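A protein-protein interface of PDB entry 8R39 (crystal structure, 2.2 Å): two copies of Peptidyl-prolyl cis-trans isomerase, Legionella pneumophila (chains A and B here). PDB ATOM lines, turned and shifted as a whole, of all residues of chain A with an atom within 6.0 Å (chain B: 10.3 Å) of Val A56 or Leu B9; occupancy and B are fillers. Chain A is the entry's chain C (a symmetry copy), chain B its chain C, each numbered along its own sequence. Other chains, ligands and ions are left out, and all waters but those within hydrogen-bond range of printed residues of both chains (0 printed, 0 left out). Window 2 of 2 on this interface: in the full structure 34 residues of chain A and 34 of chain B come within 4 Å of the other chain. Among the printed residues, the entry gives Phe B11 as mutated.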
ATOM      1  N   ILE A  26       3.417 -36.022 -32.035  1.00  0.00           N
ATOM      2  CA  ILE A  26       4.257 -35.312 -31.027  1.00  0.00           C
ATOM      3  C   ILE A  26       5.565 -36.101 -30.837  1.00  0.00           C
ATOM      4  O   ILE A  26       5.481 -37.261 -30.410  1.00  0.00           O
ATOM      5  CB  ILE A  26       3.466 -35.124 -29.721  1.00  0.00           C
ATOM      6  CG1 ILE A  26       2.233 -34.248 -29.923  1.00  0.00           C
ATOM      7  CG2 ILE A  26       4.356 -34.573 -28.610  1.00  0.00           C
ATOM      8  CD1 ILE A  26       1.051 -34.654 -29.068  1.00  0.00           C
ATOM      9  N   ASP A  27       6.710 -35.507 -31.174  1.00  0.00           N
ATOM     10  CA  ASP A  27       8.044 -36.153 -31.025  1.00  0.00           C
ATOM     11  C   ASP A  27       8.560 -35.891 -29.613  1.00  0.00           C
ATOM     12  O   ASP A  27       8.640 -34.710 -29.243  1.00  0.00           O
ATOM     13  CB  ASP A  27       9.028 -35.668 -32.072  1.00  0.00           C
ATOM     14  CG  ASP A  27      10.329 -36.447 -32.193  1.00  0.00           C
ATOM     15  OD1 ASP A  27      10.440 -37.521 -31.572  1.00  0.00           O
ATOM     16  OD2 ASP A  27      11.226 -35.973 -32.916  1.00  0.00           O
ATOM     17  N   VAL A  28       8.916 -36.937 -28.874  1.00  0.00           N
ATOM     18  CA  VAL A  28       9.331 -36.812 -27.451  1.00  0.00           C
ATOM     19  C   VAL A  28      10.486 -37.765 -27.136  1.00  0.00           C
ATOM     20  O   VAL A  28      10.497 -38.851 -27.728  1.00  0.00           O
ATOM     21  CB  VAL A  28       8.095 -37.128 -26.589  1.00  0.00           C
ATOM     22  CG1 VAL A  28       8.456 -37.476 -25.152  1.00  0.00           C
ATOM     23  CG2 VAL A  28       7.073 -36.005 -26.626  1.00  0.00           C
ATOM     24  N   LEU A  48      15.484 -26.886 -15.182  1.00  0.00           N
ATOM     25  CA  LEU A  48      14.791 -25.713 -15.760  1.00  0.00           C
ATOM     26  C   LEU A  48      14.002 -25.015 -14.652  1.00  0.00           C
ATOM     27  O   LEU A  48      13.505 -25.717 -13.764  1.00  0.00           O
ATOM     28  CB  LEU A  48      13.871 -26.141 -16.898  1.00  0.00           C
ATOM     29  CG  LEU A  48      14.546 -26.590 -18.189  1.00  0.00           C
ATOM     30  CD1 LEU A  48      13.534 -27.344 -19.011  1.00  0.00           C
ATOM     31  CD2 LEU A  48      15.080 -25.396 -18.935  1.00  0.00           C
ATOM     32  N   GLN A  51       9.396 -20.873 -14.699  1.00  0.00           N
ATOM     33  CA  GLN A  51       9.025 -19.971 -15.816  1.00  0.00           C
ATOM     34  C   GLN A  51       9.536 -20.557 -17.134  1.00  0.00           C
ATOM     35  O   GLN A  51       8.777 -20.525 -18.106  1.00  0.00           O
ATOM     36  CB  GLN A  51       9.605 -18.578 -15.593  1.00  0.00           C
ATOM     37  CG  GLN A  51       9.105 -17.518 -16.568  1.00  0.00           C
ATOM     38  CD  GLN A  51       7.613 -17.289 -16.490  1.00  0.00           C
ATOM     39  OE1 GLN A  51       7.011 -17.289 -15.410  1.00  0.00           O
ATOM     40  NE2 GLN A  51       7.001 -17.089 -17.646  1.00  0.00           N
ATOM     41  N   GLN A  52      10.766 -21.063 -17.164  1.00  0.00           N
ATOM     42  CA  GLN A  52      11.324 -21.707 -18.373  1.00  0.00           C
ATOM     43  C   GLN A  52      10.388 -22.833 -18.833  1.00  0.00           C
ATOM     44  O   GLN A  52      10.084 -22.890 -20.032  1.00  0.00           O
ATOM     45  CB  GLN A  52      12.698 -22.302 -18.098  1.00  0.00           C
ATOM     46  CG  GLN A  52      13.857 -21.335 -18.283  1.00  0.00           C
ATOM     47  CD  GLN A  52      15.193 -21.998 -18.043  1.00  0.00           C
ATOM     48  OE1 GLN A  52      15.527 -22.393 -16.923  1.00  0.00           O
ATOM     49  NE2 GLN A  52      15.959 -22.158 -19.110  1.00  0.00           N
ATOM     50  N   MET A  53       9.957 -23.682 -17.903  1.00  0.00           N
ATOM     51  CA  MET A  53       9.099 -24.843 -18.230  1.00  0.00           C
ATOM     52  C   MET A  53       7.703 -24.351 -18.616  1.00  0.00           C
ATOM     53  O   MET A  53       7.092 -24.991 -19.456  1.00  0.00           O
ATOM     54  CB  MET A  53       9.006 -25.785 -17.031  1.00  0.00           C
ATOM     55  CG  MET A  53      10.271 -26.564 -16.756  1.00  0.00           C
ATOM     56  SD  MET A  53      10.052 -27.774 -15.437  1.00  0.00           S
ATOM     57  CE  MET A  53      10.022 -26.661 -14.026  1.00  0.00           C
ATOM     58  N   LYS A  54       7.231 -23.266 -18.008  1.00  0.00           N
ATOM     59  CA  LYS A  54       5.899 -22.698 -18.323  1.00  0.00           C
ATOM     60  C   LYS A  54       5.951 -22.079 -19.719  1.00  0.00           C
ATOM     61  O   LYS A  54       4.928 -22.089 -20.385  1.00  0.00           O
ATOM     62  CB  LYS A  54       5.486 -21.669 -17.271  1.00  0.00           C
ATOM     63  CG  LYS A  54       4.082 -21.119 -17.397  1.00  0.00           C
ATOM     64  CD  LYS A  54       3.827 -19.935 -16.478  1.00  0.00           C
ATOM     65  CE  LYS A  54       4.393 -18.682 -17.048  1.00  0.00           C
ATOM     66  NZ  LYS A  54       3.444 -18.004 -17.928  1.00  0.00           N
ATOM     67  N   ASP A  55       7.106 -21.577 -20.130  1.00  0.00           N
ATOM     68  CA  ASP A  55       7.279 -20.970 -21.470  1.00  0.00           C
ATOM     69  C   ASP A  55       7.277 -22.076 -22.527  1.00  0.00           C
ATOM     70  O   ASP A  55       6.641 -21.871 -23.556  1.00  0.00           O
ATOM     71  CB  ASP A  55       8.550 -20.144 -21.527  1.00  0.00           C
ATOM     72  CG  ASP A  55       8.476 -18.746 -20.930  1.00  0.00           C
ATOM     73  OD1 ASP A  55       7.355 -18.230 -20.762  1.00  0.00           O
ATOM     74  OD2 ASP A  55       9.549 -18.180 -20.649  1.00  0.00           O
ATOM     75  N   VAL A  56       7.980 -23.182 -22.293  1.00  0.00           N
ATOM     76  CA  VAL A  56       8.050 -24.336 -23.237  1.00  0.00           C
ATOM     77  C   VAL A  56       6.657 -24.940 -23.462  1.00  0.00           C
ATOM     78  O   VAL A  56       6.312 -25.187 -24.624  1.00  0.00           O
ATOM     79  CB  VAL A  56       9.032 -25.369 -22.659  1.00  0.00           C
ATOM     80  CG1 VAL A  56       8.831 -26.761 -23.238  1.00  0.00           C
ATOM     81  CG2 VAL A  56      10.474 -24.922 -22.826  1.00  0.00           C
ATOM     82  N   LEU A  57       5.882 -25.126 -22.405  1.00  0.00           N
ATOM     83  CA  LEU A  57       4.568 -25.799 -22.512  1.00  0.00           C
ATOM     84  C   LEU A  57       3.516 -24.888 -23.165  1.00  0.00           C
ATOM     85  O   LEU A  57       2.710 -25.411 -23.940  1.00  0.00           O
ATOM     86  CB  LEU A  57       4.172 -26.248 -21.112  1.00  0.00           C
ATOM     87  CG  LEU A  57       5.016 -27.373 -20.511  1.00  0.00           C
ATOM     88  CD1 LEU A  57       4.638 -27.600 -19.064  1.00  0.00           C
ATOM     89  CD2 LEU A  57       4.872 -28.646 -21.314  1.00  0.00           C
ATOM     90  N   ASN A  58       3.526 -23.590 -22.871  1.00  0.00           N
ATOM     91  CA  ASN A  58       2.554 -22.630 -23.460  1.00  0.00           C
ATOM     92  C   ASN A  58       2.810 -22.564 -24.966  1.00  0.00           C
ATOM     93  O   ASN A  58       1.828 -22.557 -25.730  1.00  0.00           O
ATOM     94  CB  ASN A  58       2.619 -21.255 -22.805  1.00  0.00           C
ATOM     95  CG  ASN A  58       2.008 -21.209 -21.424  1.00  0.00           C
ATOM     96  OD1 ASN A  58       1.093 -21.975 -21.106  1.00  0.00           O
ATOM     97  ND2 ASN A  58       2.490 -20.301 -20.590  1.00  0.00           N
ATOM     98  N   LYS A  59       4.075 -22.560 -25.378  1.00  0.00           N
ATOM     99  CA  LYS A  59       4.423 -22.552 -26.817  1.00  0.00           C
ATOM    100  C   LYS A  59       3.933 -23.857 -27.453  1.00  0.00           C
ATOM    101  O   LYS A  59       3.372 -23.791 -28.549  1.00  0.00           O
ATOM    102  CB  LYS A  59       5.929 -22.399 -27.013  1.00  0.00           C
ATOM    103  CG  LYS A  59       6.448 -22.900 -28.345  1.00  0.00           C
ATOM    104  CD  LYS A  59       7.829 -22.371 -28.690  1.00  0.00           C
ATOM    105  CE  LYS A  59       8.114 -22.529 -30.139  1.00  0.00           C
ATOM    106  NZ  LYS A  59       8.902 -21.397 -30.622  1.00  0.00           N
ATOM    107  N   PHE A  60       4.150 -24.990 -26.793  1.00  0.00           N
ATOM    108  CA  PHE A  60       3.750 -26.305 -27.347  1.00  0.00           C
ATOM    109  C   PHE A  60       2.257 -26.290 -27.601  1.00  0.00           C
ATOM    110  O   PHE A  60       1.845 -26.679 -28.696  1.00  0.00           O
ATOM    111  CB  PHE A  60       4.119 -27.456 -26.412  1.00  0.00           C
ATOM    112  CG  PHE A  60       3.471 -28.789 -26.750  1.00  0.00           C
ATOM    113  CD1 PHE A  60       4.001 -29.615 -27.730  1.00  0.00           C
ATOM    114  CD2 PHE A  60       2.336 -29.214 -26.076  1.00  0.00           C
ATOM    115  CE1 PHE A  60       3.409 -30.831 -28.028  1.00  0.00           C
ATOM    116  CE2 PHE A  60       1.748 -30.430 -26.378  1.00  0.00           C
ATOM    117  CZ  PHE A  60       2.285 -31.235 -27.353  1.00  0.00           C
ATOM    118  N   GLN A  61       1.470 -25.837 -26.633  1.00  0.00           N
ATOM    119  CA  GLN A  61      -0.008 -25.852 -26.760  1.00  0.00           C
ATOM    120  C   GLN A  61      -0.428 -24.969 -27.949  1.00  0.00           C
ATOM    121  O   GLN A  61      -1.323 -25.391 -28.693  1.00  0.00           O
ATOM    122  CB  GLN A  61      -0.655 -25.430 -25.442  1.00  0.00           C
ATOM    123  CG  GLN A  61      -0.575 -26.487 -24.346  1.00  0.00           C
ATOM    124  CD  GLN A  61      -1.404 -27.718 -24.638  1.00  0.00           C
ATOM    125  OE1 GLN A  61      -2.578 -27.635 -25.010  1.00  0.00           O
ATOM    126  NE2 GLN A  61      -0.794 -28.880 -24.466  1.00  0.00           N
ATOM    127  N   SER B   1      20.632 -34.800 -20.973  1.00  0.00           N
ATOM    128  CA  SER B   1      20.916 -33.619 -21.831  1.00  0.00           C
ATOM    129  C   SER B   1      19.634 -32.839 -22.121  1.00  0.00           C
ATOM    130  O   SER B   1      18.697 -33.470 -22.637  1.00  0.00           O
ATOM    131  CB  SER B   1      21.564 -34.024 -23.123  1.00  0.00           C
ATOM    132  OG  SER B   1      21.540 -32.961 -24.065  1.00  0.00           O
ATOM    133  N   LEU B   2      19.609 -31.540 -21.817  1.00  0.00           N
ATOM    134  CA  LEU B   2      18.465 -30.660 -22.151  1.00  0.00           C
ATOM    135  C   LEU B   2      19.031 -29.604 -23.104  1.00  0.00           C
ATOM    136  O   LEU B   2      18.882 -28.417 -22.819  1.00  0.00           O
ATOM    137  CB  LEU B   2      17.832 -30.069 -20.896  1.00  0.00           C
ATOM    138  CG  LEU B   2      17.203 -31.061 -19.916  1.00  0.00           C
ATOM    139  CD1 LEU B   2      16.366 -30.292 -18.922  1.00  0.00           C
ATOM    140  CD2 LEU B   2      16.346 -32.108 -20.586  1.00  0.00           C
ATOM    141  N   ALA B   3      19.688 -30.035 -24.177  1.00  0.00           N
ATOM    142  CA  ALA B   3      20.308 -29.130 -25.163  1.00  0.00           C
ATOM    143  C   ALA B   3      19.308 -28.740 -26.240  1.00  0.00           C
ATOM    144  O   ALA B   3      19.402 -27.592 -26.703  1.00  0.00           O
ATOM    145  CB  ALA B   3      21.474 -29.828 -25.784  1.00  0.00           C
ATOM    146  N   THR B   4      18.404 -29.638 -26.624  1.00  0.00           N
ATOM    147  CA  THR B   4      17.458 -29.416 -27.733  1.00  0.00           C
ATOM    148  C   THR B   4      16.102 -29.037 -27.205  1.00  0.00           C
ATOM    149  O   THR B   4      15.849 -29.268 -26.016  1.00  0.00           O
ATOM    150  CB  THR B   4      17.395 -30.686 -28.575  1.00  0.00           C
ATOM    151  OG1 THR B   4      16.612 -31.618 -27.841  1.00  0.00           O
ATOM    152  CG2 THR B   4      18.770 -31.272 -28.835  1.00  0.00           C
ATOM    153  N   ASP B   5      15.262 -28.461 -28.057  1.00  0.00           N
ATOM    154  CA  ASP B   5      13.871 -28.127 -27.673  1.00  0.00           C
ATOM    155  C   ASP B   5      13.105 -29.420 -27.392  1.00  0.00           C
ATOM    156  O   ASP B   5      12.218 -29.385 -26.531  1.00  0.00           O
ATOM    157  CB  ASP B   5      13.165 -27.336 -28.755  1.00  0.00           C
ATOM    158  CG  ASP B   5      13.685 -25.938 -29.045  1.00  0.00           C
ATOM    159  OD1 ASP B   5      14.407 -25.374 -28.202  1.00  0.00           O
ATOM    160  OD2 ASP B   5      13.343 -25.428 -30.119  1.00  0.00           O
ATOM    161  N   LYS B   6      13.429 -30.502 -28.098  1.00  0.00           N
ATOM    162  CA  LYS B   6      12.773 -31.817 -27.888  1.00  0.00           C
ATOM    163  C   LYS B   6      13.030 -32.280 -26.443  1.00  0.00           C
ATOM    164  O   LYS B   6      12.065 -32.654 -25.767  1.00  0.00           O
ATOM    165  CB  LYS B   6      13.294 -32.811 -28.930  1.00  0.00           C
ATOM    166  CG  LYS B   6      12.714 -34.208 -28.869  1.00  0.00           C
ATOM    167  CD  LYS B   6      13.258 -35.108 -29.967  1.00  0.00           C
ATOM    168  CE  LYS B   6      12.764 -36.506 -29.855  1.00  0.00           C
ATOM    169  NZ  LYS B   6      13.173 -37.301 -31.012  1.00  0.00           N
ATOM    170  N   ASP B   7      14.277 -32.221 -25.990  1.00  0.00           N
ATOM    171  CA  ASP B   7      14.654 -32.645 -24.621  1.00  0.00           C
ATOM    172  C   ASP B   7      13.948 -31.775 -23.579  1.00  0.00           C
ATOM    173  O   ASP B   7      13.442 -32.330 -22.606  1.00  0.00           O
ATOM    174  CB  ASP B   7      16.156 -32.554 -24.454  1.00  0.00           C
ATOM    175  CG  ASP B   7      16.994 -33.483 -25.318  1.00  0.00           C
ATOM    176  OD1 ASP B   7      16.553 -34.624 -25.557  1.00  0.00           O
ATOM    177  OD2 ASP B   7      18.086 -33.055 -25.739  1.00  0.00           O
ATOM    178  N   LYS B   8      13.915 -30.467 -23.783  1.00  0.00           N
ATOM    179  CA  LYS B   8      13.347 -29.526 -22.793  1.00  0.00           C
ATOM    180  C   LYS B   8      11.833 -29.712 -22.701  1.00  0.00           C
ATOM    181  O   LYS B   8      11.321 -29.671 -21.584  1.00  0.00           O
ATOM    182  CB  LYS B   8      13.753 -28.115 -23.212  1.00  0.00           C
ATOM    183  CG  LYS B   8      15.198 -27.767 -22.944  1.00  0.00           C
ATOM    184  CD  LYS B   8      15.545 -26.384 -23.467  1.00  0.00           C
ATOM    185  CE  LYS B   8      17.010 -26.187 -23.568  1.00  0.00           C
ATOM    186  NZ  LYS B   8      17.330 -24.828 -23.994  1.00  0.00           N
ATOM    187  N   LEU B   9      11.161 -29.924 -23.827  1.00  0.00           N
ATOM    188  CA  LEU B   9       9.698 -30.166 -23.840  1.00  0.00           C
ATOM    189  C   LEU B   9       9.440 -31.491 -23.122  1.00  0.00           C
ATOM    190  O   LEU B   9       8.515 -31.546 -22.305  1.00  0.00           O
ATOM    191  CB  LEU B   9       9.146 -30.194 -25.265  1.00  0.00           C
ATOM    192  CG  LEU B   9       7.760 -30.820 -25.427  1.00  0.00           C
ATOM    193  CD1 LEU B   9       6.718 -30.005 -24.700  1.00  0.00           C
ATOM    194  CD2 LEU B   9       7.406 -30.954 -26.889  1.00  0.00           C
ATOM    195  N   SER B  10      10.251 -32.498 -23.414  1.00  0.00           N
ATOM    196  CA  SER B  10      10.084 -33.845 -22.828  1.00  0.00           C
ATOM    197  C   SER B  10      10.273 -33.776 -21.307  1.00  0.00           C
ATOM    198  O   SER B  10       9.436 -34.337 -20.590  1.00  0.00           O
ATOM    199  CB  SER B  10      11.023 -34.806 -23.490  1.00  0.00           C
ATOM    200  OG  SER B  10      10.678 -35.014 -24.850  1.00  0.00           O
ATOM    201  N   PHE B  11      11.286 -33.056 -20.844  1.00  0.00           N
ATOM    202  CA  PHE B  11      11.587 -32.917 -19.400  1.00  0.00           C
ATOM    203  C   PHE B  11      10.474 -32.161 -18.725  1.00  0.00           C
ATOM    204  O   PHE B  11      10.103 -32.524 -17.608  1.00  0.00           O
ATOM    205  CB  PHE B  11      12.921 -32.183 -19.277  1.00  0.00           C
ATOM    206  CG  PHE B  11      13.317 -31.796 -17.863  1.00  0.00           C
ATOM    207  CD1 PHE B  11      12.785 -30.669 -17.257  1.00  0.00           C
ATOM    208  CD2 PHE B  11      14.226 -32.561 -17.149  1.00  0.00           C
ATOM    209  CE1 PHE B  11      13.144 -30.325 -15.968  1.00  0.00           C
ATOM    210  CE2 PHE B  11      14.586 -32.209 -15.862  1.00  0.00           C
ATOM    211  CZ  PHE B  11      14.045 -31.093 -15.275  1.00  0.00           C
ATOM    212  N   SER B  12       9.956 -31.136 -19.391  1.00  0.00           N
ATOM    213  CA  SER B  12       8.914 -30.268 -18.806  1.00  0.00           C
ATOM    214  C   SER B  12       7.606 -31.050 -18.661  1.00  0.00           C
ATOM    215  O   SER B  12       6.924 -30.861 -17.642  1.00  0.00           O
ATOM    216  CB  SER B  12       8.764 -29.042 -19.629  1.00  0.00           C
ATOM    217  OG  SER B  12       9.895 -28.197 -19.487  1.00  0.00           O
ATOM    218  N   ILE B  13       7.304 -31.936 -19.604  1.00  0.00           N
ATOM    219  CA  ILE B  13       6.078 -32.782 -19.522  1.00  0.00           C
ATOM    220  C   ILE B  13       6.249 -33.760 -18.352  1.00  0.00           C
ATOM    221  O   ILE B  13       5.311 -33.888 -17.556  1.00  0.00           O
ATOM    222  CB  ILE B  13       5.809 -33.495 -20.860  1.00  0.00           C
ATOM    223  CG1 ILE B  13       5.387 -32.514 -21.948  1.00  0.00           C
ATOM    224  CG2 ILE B  13       4.779 -34.610 -20.682  1.00  0.00           C
ATOM    225  CD1 ILE B  13       5.653 -32.998 -23.359  1.00  0.00           C
ATOM    226  N   GLY B  14       7.419 -34.379 -18.234  1.00  0.00           N
ATOM    227  CA  GLY B  14       7.692 -35.342 -17.159  1.00  0.00           C
ATOM    228  C   GLY B  14       7.582 -34.697 -15.802  1.00  0.00           C
ATOM    229  O   GLY B  14       7.030 -35.334 -14.897  1.00  0.00           O
ATOM    230  N   ALA B  15       8.074 -33.474 -15.658  1.00  0.00           N
ATOM    231  CA  ALA B  15       8.068 -32.764 -14.366  1.00  0.00           C
ATOM    232  C   ALA B  15       6.628 -32.482 -13.947  1.00  0.00           C
ATOM    233  O   ALA B  15       6.315 -32.656 -12.766  1.00  0.00           O
ATOM    234  CB  ALA B  15       8.867 -31.505 -14.501  1.00  0.00           C
ATOM    235  N   ASP B  16       5.782 -32.078 -14.891  1.00  0.00           N
ATOM    236  CA  ASP B  16       4.359 -31.772 -14.611  1.00  0.00           C
ATOM    237  C   ASP B  16       3.655 -33.047 -14.161  1.00  0.00           C
ATOM    238  O   ASP B  16       2.904 -32.987 -13.175  1.00  0.00           O
ATOM    239  CB  ASP B  16       3.681 -31.166 -15.822  1.00  0.00           C
ATOM    240  CG  ASP B  16       2.233 -30.755 -15.603  1.00  0.00           C
ATOM    241  OD1 ASP B  16       2.016 -29.674 -15.025  1.00  0.00           O
ATOM    242  OD2 ASP B  16       1.341 -31.530 -16.000  1.00  0.00           O
ATOM    243  N   LEU B  17       3.915 -34.160 -14.838  1.00  0.00           N
ATOM    244  CA  LEU B  17       3.312 -35.463 -14.471  1.00  0.00           C
ATOM    245  C   LEU B  17       3.765 -35.837 -13.060  1.00  0.00           C
ATOM    246  O   LEU B  17       2.917 -36.259 -12.274  1.00  0.00           O
ATOM    247  CB  LEU B  17       3.733 -36.519 -15.484  1.00  0.00           C
ATOM    248  CG  LEU B  17       3.108 -36.405 -16.873  1.00  0.00           C
ATOM    249  CD1 LEU B  17       4.030 -36.983 -17.920  1.00  0.00           C
ATOM    250  CD2 LEU B  17       1.769 -37.098 -16.897  1.00  0.00           C
ATOM    251  N   MET B  37       6.451 -46.263 -23.078  1.00  0.00           N
ATOM    252  CA  MET B  37       6.308 -45.132 -24.021  1.00  0.00           C
ATOM    253  C   MET B  37       7.162 -45.406 -25.262  1.00  0.00           C
ATOM    254  O   MET B  37       6.654 -45.217 -26.375  1.00  0.00           O
ATOM    255  CB  MET B  37       6.746 -43.829 -23.354  1.00  0.00           C
ATOM    256  CG  MET B  37       6.431 -42.593 -24.165  1.00  0.00           C
ATOM    257  SD  MET B  37       6.892 -41.061 -23.335  1.00  0.00           S
ATOM    258  CE  MET B  37       5.926 -41.214 -21.828  1.00  0.00           C
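Of the 15 printed residues of chain A, 7 touch a printed residue of chain B.
Along chain A the printed residues that touch a printed residue of chain B span positions 27 to 60.
Hydrophobic or aromatic side chains of chain B within 4 Å of the printed part of chain A: Leu B9, Phe B11 and Ile B13.
Among the printed residues, 9 pairs touch across the chains.
The side-chain hydroxyl (OG1) of Thr B4 lies close to the backbone NH (N) of Lys B6, at 3.4 Å.
The side-chain hydroxyl (OG) of Ser B10 lies within hydrogen-bond range of the backbone carbonyl oxygen (O) of Lys B6 (2.9 Å).
The side-chain hydroxyl (OG) of Ser B12 is in hydrogen-bond range of the backbone carbonyl oxygen (O) of Lys B8 (2.9 Å).
Lys B6 touches Val A28.
Ser B10 touches Val A28 (OG to CG1, 3.3 Å).
Phe B11 touches Leu A48 (CD1 to CD1, 3.8 Å).
Leu A48 touches Ser B12 (CD1 to OG, 3.8 Å).
Met A53 touches Ser B12.
Leu B9 touches Val A56.
Leu A57 touches Ile B13 (CD2 to CG1, 3.95 Å).
Phe A60 touches Leu B9.
The side-chain amino group (NZ) of Lys B6 lies within salt-bridge range of the side-chain carboxylate (OD1) of Asp A27, at 2.8 Å.
Of the printed residues of chain B, Asp A27 touches Lys B6 (2.8 Å).
Printed residues of chain B within 4 Å of Leu A48: Phe B11 (3.8 Å) and Ser B12 (3.8 Å).
No residue of chain B comes within 4 Å of Asp A55.
Of the printed residues of chain B, Val A56 touches Leu B9 (3.6 Å).
Phe A60 touches one residue of chain B.
Leu B2 touches none of the printed residues of chain A.
Thr B4 touches none of the printed residues of chain A.
Of the printed residues of chain A, Lys B6 touches Asp A27 (2.8 Å) and Val A28 (3.8 Å).
Of the printed residues of chain A, Leu B9 touches Val A56 and Phe A60.
The nearest printed residue of chain B that does not touch Val A56 is Ser B12 (4.2 Å).
The nearest residue of chain A that does not touch Leu B9 is Leu A57 (4.1 Å).
The nearest printed residue of chain B that does not touch Leu A48 is Leu B2 (4.1 Å).
No position is printed for both chains.
Of the 9 pairs that touch across the chains among the printed residues, none has its exchanged pair printed and touching as well.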
